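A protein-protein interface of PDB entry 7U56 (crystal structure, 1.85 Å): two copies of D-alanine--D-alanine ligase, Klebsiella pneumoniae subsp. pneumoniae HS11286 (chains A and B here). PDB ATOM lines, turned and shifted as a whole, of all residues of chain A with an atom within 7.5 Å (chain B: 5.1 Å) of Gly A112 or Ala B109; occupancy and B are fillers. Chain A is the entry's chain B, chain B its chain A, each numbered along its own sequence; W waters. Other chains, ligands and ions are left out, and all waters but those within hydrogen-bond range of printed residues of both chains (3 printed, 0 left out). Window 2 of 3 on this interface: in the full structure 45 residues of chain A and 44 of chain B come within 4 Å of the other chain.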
ATOM      1  N   ALA A  96      25.249  16.191   0.857  1.00  0.00           N
ATOM      2  CA  ALA A  96      24.743  15.015   0.160  1.00  0.00           C
ATOM      3  C   ALA A  96      23.225  14.984   0.301  1.00  0.00           C
ATOM      4  O   ALA A  96      22.659  15.570   1.234  1.00  0.00           O
ATOM      5  CB  ALA A  96      25.354  13.709   0.705  1.00  0.00           C
ATOM      6  N   GLN A  97      22.570  14.293  -0.635  1.00  0.00           N
ATOM      7  CA  GLN A  97      21.124  14.098  -0.601  1.00  0.00           C
ATOM      8  C   GLN A  97      20.813  12.622  -0.416  1.00  0.00           C
ATOM      9  O   GLN A  97      21.391  11.769  -1.088  1.00  0.00           O
ATOM     10  CB  GLN A  97      20.432  14.600  -1.874  1.00  0.00           C
ATOM     11  CG  GLN A  97      18.999  14.051  -1.999  1.00  0.00           C
ATOM     12  CD  GLN A  97      18.370  14.491  -3.279  1.00  0.00           C
ATOM     13  OE1 GLN A  97      19.070  14.722  -4.263  1.00  0.00           O
ATOM     14  NE2 GLN A  97      17.049  14.619  -3.286  1.00  0.00           N
ATOM     15  N   ILE A  98      19.895  12.323   0.494  1.00  0.00           N
ATOM     16  CA  ILE A  98      19.358  10.974   0.626  1.00  0.00           C
ATOM     17  C   ILE A  98      18.088  10.935  -0.214  1.00  0.00           C
ATOM     18  O   ILE A  98      17.089  11.565   0.168  1.00  0.00           O
ATOM     19  CB  ILE A  98      19.102  10.598   2.088  1.00  0.00           C
ATOM     20  CG1 ILE A  98      20.443  10.570   2.828  1.00  0.00           C
ATOM     21  CG2 ILE A  98      18.425   9.243   2.169  1.00  0.00           C
ATOM     22  CD1 ILE A  98      20.348  11.034   4.238  1.00  0.00           C
ATOM     23  N   ARG A 101      13.835  10.657   0.804  1.00  0.00           N
ATOM     24  CA  ARG A 101      13.469  11.198   2.103  1.00  0.00           C
ATOM     25  C   ARG A 101      12.628  12.462   1.933  1.00  0.00           C
ATOM     26  O   ARG A 101      12.844  13.266   1.022  1.00  0.00           O
ATOM     27  CB  ARG A 101      14.713  11.522   2.924  1.00  0.00           C
ATOM     28  CG  ARG A 101      15.269  10.367   3.733  1.00  0.00           C
ATOM     29  CD  ARG A 101      16.308  10.911   4.709  1.00  0.00           C
ATOM     30  NE  ARG A 101      16.868   9.893   5.587  1.00  0.00           N
ATOM     31  CZ  ARG A 101      17.810  10.124   6.496  1.00  0.00           C
ATOM     32  NH1 ARG A 101      18.324  11.329   6.673  1.00  0.00           N
ATOM     33  NH2 ARG A 101      18.254   9.119   7.244  1.00  0.00           N
ATOM     34  N   GLN A 104      14.930  15.532   6.638  1.00  0.00           N
ATOM     35  CA  GLN A 104      16.362  15.280   6.751  1.00  0.00           C
ATOM     36  C   GLN A 104      16.923  14.812   5.411  1.00  0.00           C
ATOM     37  O   GLN A 104      17.683  13.843   5.330  1.00  0.00           O
ATOM     38  CB  GLN A 104      16.650  14.267   7.862  1.00  0.00           C
ATOM     39  CG  GLN A 104      16.087  14.694   9.218  1.00  0.00           C
ATOM     40  CD  GLN A 104      16.596  13.844  10.363  1.00  0.00           C
ATOM     41  OE1 GLN A 104      16.961  12.680  10.177  1.00  0.00           O
ATOM     42  NE2 GLN A 104      16.632  14.428  11.565  1.00  0.00           N
ATOM     43  N   LEU A 106      18.911  16.486   3.230  1.00  0.00           N
ATOM     44  CA  LEU A 106      20.283  16.895   2.962  1.00  0.00           C
ATOM     45  C   LEU A 106      21.100  16.669   4.219  1.00  0.00           C
ATOM     46  O   LEU A 106      20.670  17.044   5.321  1.00  0.00           O
ATOM     47  CB  LEU A 106      20.371  18.367   2.556  1.00  0.00           C
ATOM     48  CG  LEU A 106      19.491  18.777   1.376  1.00  0.00           C
ATOM     49  CD1 LEU A 106      19.600  20.278   1.174  1.00  0.00           C
ATOM     50  CD2 LEU A 106      19.933  18.009   0.137  1.00  0.00           C
ATOM     51  N   ILE A 107      22.262  16.050   4.056  1.00  0.00           N
ATOM     52  CA  ILE A 107      23.170  15.832   5.166  1.00  0.00           C
ATOM     53  C   ILE A 107      24.499  16.527   4.886  1.00  0.00           C
ATOM     54  O   ILE A 107      24.873  16.820   3.742  1.00  0.00           O
ATOM     55  CB  ILE A 107      23.410  14.339   5.448  1.00  0.00           C
ATOM     56  CG1 ILE A 107      24.049  13.665   4.222  1.00  0.00           C
ATOM     57  CG2 ILE A 107      22.099  13.633   5.899  1.00  0.00           C
ATOM     58  CD1 ILE A 107      24.583  12.275   4.517  1.00  0.00           C
ATOM     59  N   ASN A 108      25.203  16.786   5.975  1.00  0.00           N
ATOM     60  CA  ASN A 108      26.635  17.058   6.001  1.00  0.00           C
ATOM     61  C   ASN A 108      27.356  15.758   5.664  1.00  0.00           C
ATOM     62  O   ASN A 108      27.330  14.818   6.460  1.00  0.00           O
ATOM     63  CB  ASN A 108      26.959  17.558   7.414  1.00  0.00           C
ATOM     64  CG  ASN A 108      28.422  17.875   7.648  1.00  0.00           C
ATOM     65  OD1 ASN A 108      29.333  17.314   7.027  1.00  0.00           O
ATOM     66  ND2 ASN A 108      28.654  18.761   8.615  1.00  0.00           N
ATOM     67  N   ALA A 109      27.947  15.664   4.468  1.00  0.00           N
ATOM     68  CA  ALA A 109      28.512  14.377   4.051  1.00  0.00           C
ATOM     69  C   ALA A 109      29.661  13.939   4.959  1.00  0.00           C
ATOM     70  O   ALA A 109      29.863  12.728   5.170  1.00  0.00           O
ATOM     71  CB  ALA A 109      28.979  14.447   2.590  1.00  0.00           C
ATOM     72  N   GLU A 110      30.416  14.900   5.505  1.00  0.00           N
ATOM     73  CA  GLU A 110      31.565  14.586   6.344  1.00  0.00           C
ATOM     74  C   GLU A 110      31.157  14.071   7.721  1.00  0.00           C
ATOM     75  O   GLU A 110      31.907  13.313   8.338  1.00  0.00           O
ATOM     76  CB  GLU A 110      32.452  15.828   6.510  1.00  0.00           C
ATOM     77  CG  GLU A 110      33.315  16.120   5.283  1.00  0.00           C
ATOM     78  CD  GLU A 110      32.544  16.802   4.164  1.00  0.00           C
ATOM     79  OE1 GLU A 110      31.405  17.258   4.417  1.00  0.00           O
ATOM     80  OE2 GLU A 110      33.081  16.872   3.034  1.00  0.00           O
ATOM     81  N   SER A 111      29.988  14.449   8.212  1.00  0.00           N
ATOM     82  CA  SER A 111      29.575  14.047   9.549  1.00  0.00           C
ATOM     83  C   SER A 111      28.361  13.136   9.571  1.00  0.00           C
ATOM     84  O   SER A 111      28.023  12.630  10.648  1.00  0.00           O
ATOM     85  CB  SER A 111      29.257  15.284  10.404  1.00  0.00           C
ATOM     86  OG  SER A 111      28.048  15.896   9.958  1.00  0.00           O
ATOM     87  N   GLY A 112      27.673  12.949   8.443  1.00  0.00           N
ATOM     88  CA  GLY A 112      26.438  12.194   8.423  1.00  0.00           C
ATOM     89  C   GLY A 112      25.265  12.898   9.061  1.00  0.00           C
ATOM     90  O   GLY A 112      24.169  12.337   9.088  1.00  0.00           O
ATOM     91  N   GLN A 113      25.447  14.118   9.543  1.00  0.00           N
ATOM     92  CA  GLN A 113      24.325  14.675  10.286  1.00  0.00           C
ATOM     93  C   GLN A 113      23.410  15.491   9.366  1.00  0.00           C
ATOM     94  O   GLN A 113      23.887  16.159   8.446  1.00  0.00           O
ATOM     95  CB  GLN A 113      24.851  15.553  11.435  1.00  0.00           C
ATOM     96  CG  GLN A 113      25.786  14.734  12.341  1.00  0.00           C
ATOM     97  CD  GLN A 113      26.260  15.445  13.596  1.00  0.00           C
ATOM     98  OE1 GLN A 113      26.301  16.671  13.661  1.00  0.00           O
ATOM     99  NE2 GLN A 113      26.630  14.664  14.600  1.00  0.00           N
ATOM    100  N   PRO A 114      22.101  15.463   9.599  1.00  0.00           N
ATOM    101  CA  PRO A 114      21.182  16.178   8.701  1.00  0.00           C
ATOM    102  C   PRO A 114      21.252  17.685   8.905  1.00  0.00           C
ATOM    103  O   PRO A 114      21.560  18.177   9.995  1.00  0.00           O
ATOM    104  CB  PRO A 114      19.810  15.626   9.097  1.00  0.00           C
ATOM    105  CG  PRO A 114      19.971  15.307  10.561  1.00  0.00           C
ATOM    106  CD  PRO A 114      21.385  14.762  10.681  1.00  0.00           C
ATOM    107  N   LEU A 115      21.012  18.426   7.823  1.00  0.00           N
ATOM    108  CA  LEU A 115      20.709  19.846   7.954  1.00  0.00           C
ATOM    109  C   LEU A 115      19.310  20.033   8.542  1.00  0.00           C
ATOM    110  O   LEU A 115      18.419  19.212   8.334  1.00  0.00           O
ATOM    111  CB  LEU A 115      20.775  20.540   6.598  1.00  0.00           C
ATOM    112  CG  LEU A 115      22.110  20.592   5.867  1.00  0.00           C
ATOM    113  CD1 LEU A 115      22.018  21.559   4.659  1.00  0.00           C
ATOM    114  CD2 LEU A 115      23.215  21.005   6.800  1.00  0.00           C
ATOM    115  N   THR B  94      21.736   3.091   4.259  1.00  0.00           N
ATOM    116  CA  THR B  94      21.097   4.247   3.656  1.00  0.00           C
ATOM    117  C   THR B  94      22.072   4.827   2.645  1.00  0.00           C
ATOM    118  O   THR B  94      23.237   5.043   2.978  1.00  0.00           O
ATOM    119  CB  THR B  94      20.773   5.288   4.721  1.00  0.00           C
ATOM    120  OG1 THR B  94      19.947   4.706   5.745  1.00  0.00           O
ATOM    121  CG2 THR B  94      20.064   6.503   4.106  1.00  0.00           C
ATOM    122  N   LEU B  95      21.630   5.048   1.407  1.00  0.00           N
ATOM    123  CA  LEU B  95      22.528   5.650   0.433  1.00  0.00           C
ATOM    124  C   LEU B  95      22.231   7.141   0.261  1.00  0.00           C
ATOM    125  O   LEU B  95      21.092   7.594   0.391  1.00  0.00           O
ATOM    126  CB  LEU B  95      22.466   4.938  -0.927  1.00  0.00           C
ATOM    127  CG  LEU B  95      21.430   5.268  -2.005  1.00  0.00           C
ATOM    128  CD1 LEU B  95      21.772   6.507  -2.836  1.00  0.00           C
ATOM    129  CD2 LEU B  95      21.237   4.047  -2.917  1.00  0.00           C
ATOM    130  N   ALA B  96      23.277   7.886  -0.068  1.00  0.00           N
ATOM    131  CA  ALA B  96      23.169   9.303  -0.377  1.00  0.00           C
ATOM    132  C   ALA B  96      23.967   9.552  -1.642  1.00  0.00           C
ATOM    133  O   ALA B  96      24.897   8.821  -1.950  1.00  0.00           O
ATOM    134  CB  ALA B  96      23.718  10.198   0.741  1.00  0.00           C
ATOM    135  N   ILE B 107      27.364   7.307  -1.560  1.00  0.00           N
ATOM    136  CA  ILE B 107      28.030   7.008  -0.302  1.00  0.00           C
ATOM    137  C   ILE B 107      27.045   6.344   0.643  1.00  0.00           C
ATOM    138  O   ILE B 107      25.824   6.472   0.505  1.00  0.00           O
ATOM    139  CB  ILE B 107      28.633   8.275   0.357  1.00  0.00           C
ATOM    140  CG1 ILE B 107      27.537   9.292   0.668  1.00  0.00           C
ATOM    141  CG2 ILE B 107      29.706   8.901  -0.563  1.00  0.00           C
ATOM    142  CD1 ILE B 107      27.982  10.379   1.692  1.00  0.00           C
ATOM    143  N   ASN B 108      27.601   5.591   1.594  1.00  0.00           N
ATOM    144  CA  ASN B 108      26.853   5.173   2.769  1.00  0.00           C
ATOM    145  C   ASN B 108      26.543   6.433   3.571  1.00  0.00           C
ATOM    146  O   ASN B 108      27.463   7.129   3.989  1.00  0.00           O
ATOM    147  CB  ASN B 108      27.689   4.172   3.582  1.00  0.00           C
ATOM    148  CG  ASN B 108      26.977   3.654   4.813  1.00  0.00           C
ATOM    149  OD1 ASN B 108      26.367   4.402   5.575  1.00  0.00           O
ATOM    150  ND2 ASN B 108      27.061   2.339   5.020  1.00  0.00           N
ATOM    151  N   ALA B 109      25.261   6.763   3.746  1.00  0.00           N
ATOM    152  CA  ALA B 109      24.931   8.059   4.340  1.00  0.00           C
ATOM    153  C   ALA B 109      25.377   8.148   5.799  1.00  0.00           C
ATOM    154  O   ALA B 109      25.749   9.228   6.266  1.00  0.00           O
ATOM    155  CB  ALA B 109      23.431   8.327   4.235  1.00  0.00           C
ATOM    156  N   GLU B 110      25.361   7.031   6.522  1.00  0.00           N
ATOM    157  CA  GLU B 110      25.684   7.070   7.945  1.00  0.00           C
ATOM    158  C   GLU B 110      27.189   7.031   8.203  1.00  0.00           C
ATOM    159  O   GLU B 110      27.656   7.608   9.190  1.00  0.00           O
ATOM    160  CB  GLU B 110      25.009   5.909   8.660  1.00  0.00           C
ATOM    161  CG  GLU B 110      23.512   6.045   8.720  1.00  0.00           C
ATOM    162  CD  GLU B 110      22.882   4.966   9.579  1.00  0.00           C
ATOM    163  OE1 GLU B 110      23.605   4.361  10.402  1.00  0.00           O
ATOM    164  OE2 GLU B 110      21.666   4.735   9.440  1.00  0.00           O
ATOM    165  N   SER B 111      27.954   6.348   7.356  1.00  0.00           N
ATOM    166  CA  SER B 111      29.400   6.250   7.567  1.00  0.00           C
ATOM    167  C   SER B 111      30.203   7.201   6.688  1.00  0.00           C
ATOM    168  O   SER B 111      31.373   7.465   6.990  1.00  0.00           O
ATOM    169  CB  SER B 111      29.881   4.817   7.307  1.00  0.00           C
ATOM    170  OG  SER B 111      29.875   4.610   5.903  1.00  0.00           O
ATOM    171  N   GLY B 112      29.615   7.713   5.610  1.00  0.00           N
ATOM    172  CA  GLY B 112      30.340   8.520   4.655  1.00  0.00           C
ATOM    173  C   GLY B 112      31.203   7.747   3.677  1.00  0.00           C
ATOM    174  O   GLY B 112      31.805   8.361   2.787  1.00  0.00           O
HETATM  175  O   HOH W   1      23.356  10.270   7.496  1.00  0.00           O
HETATM  176  O   HOH W   2      19.881   6.285   8.346  1.00  0.00           O
HETATM  177  O   HOH W   3      28.320  10.641   6.075  1.00  0.00           O
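Of the 15 printed residues of chain A, 5 touch a printed residue of chain B. Printed residues of chain A that touch a printed residue of chain B: Ala A96, Gln A97, Ile A98, Ile A107 and Gly A112. Hydrophobic or aromatic side chains of chain A within 4 Å of the printed part of chain B: Ala A96, Ile A98 and Ile A107. Printed residues of chain B that touch a printed residue of chain A: Thr B94, Leu B95, Ala B96 and Ala B109.
Ala B96 touches its own counterpart, Ala A96. Ile A107 touches Ala B109, but with the chains exchanged Ala A109 does not touch Ile B107 (4.3 Å). Gly A112 touches Ala B109, but with the chains exchanged Ala A109 does not touch Gly B112 (4.3 Å).
O of Ala B96 sits at hydrogen-bond distance from N of Ile B107 (2.9 Å). O of Thr B94 sits at hydrogen-bond distance from N of Ala B109. The backbone carbonyl oxygen of Ala A96 lies within hydrogen-bond range of the backbone NH of Ile A107 (2.9 Å).
Gly A112 touches just one residue of chain B: Ala B109. Of the printed residues of chain A, Ala B109 touches Ile A98, Ile A107 and Gly A112. Printed residues of chain B within 4 Å of Ile A98: Thr B94 (3.7 Å), Leu B95 (3.6 Å), Ala B96 (3.9 Å) and Ala B109 (3.99 Å). Of the printed residues of chain B, Gln A97 touches Ala B96. Printed residues of chain B within 4 Å of Ala A96: Ala B96 (3.9 Å). Of the printed residues of chain A, Leu B95 touches Ile A98 (3.6 Å). The nearest residue of chain B that does not touch Gly A112 is Glu B110 (4.8 Å). The nearest printed residue of chain B that does not touch Gln A97 is Leu B95 (4.4 Å).
Among the printed residues, merely in contact across the chains: Ala A96 with Ala B96, Gln A97 with Ala B96, Ile A98 with Thr B94, Ile A98 with Leu B95, Ile A98 with Ala B96, Ile A98 with Ala B109, Ile A107 with Ala B109 and Gly A112 with Ala B109.
Water W2 lies within hydrogen-bond range of OE2 of Glu B110 (2.6 Å), OG1 of Thr B94 (3.0 Å) and NH2 of Arg A101 (3.4 Å). Water W1 bridges the backbone carbonyl oxygen of Gly A112 and the backbone carbonyl oxygen of Ala B109. Water W3 lies within hydrogen-bond range of the backbone carbonyl oxygen of Ala A109, the backbone carbonyl oxygen of Ala B109, the backbone NH of Gly B112 and the backbone NH of Gly A112.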
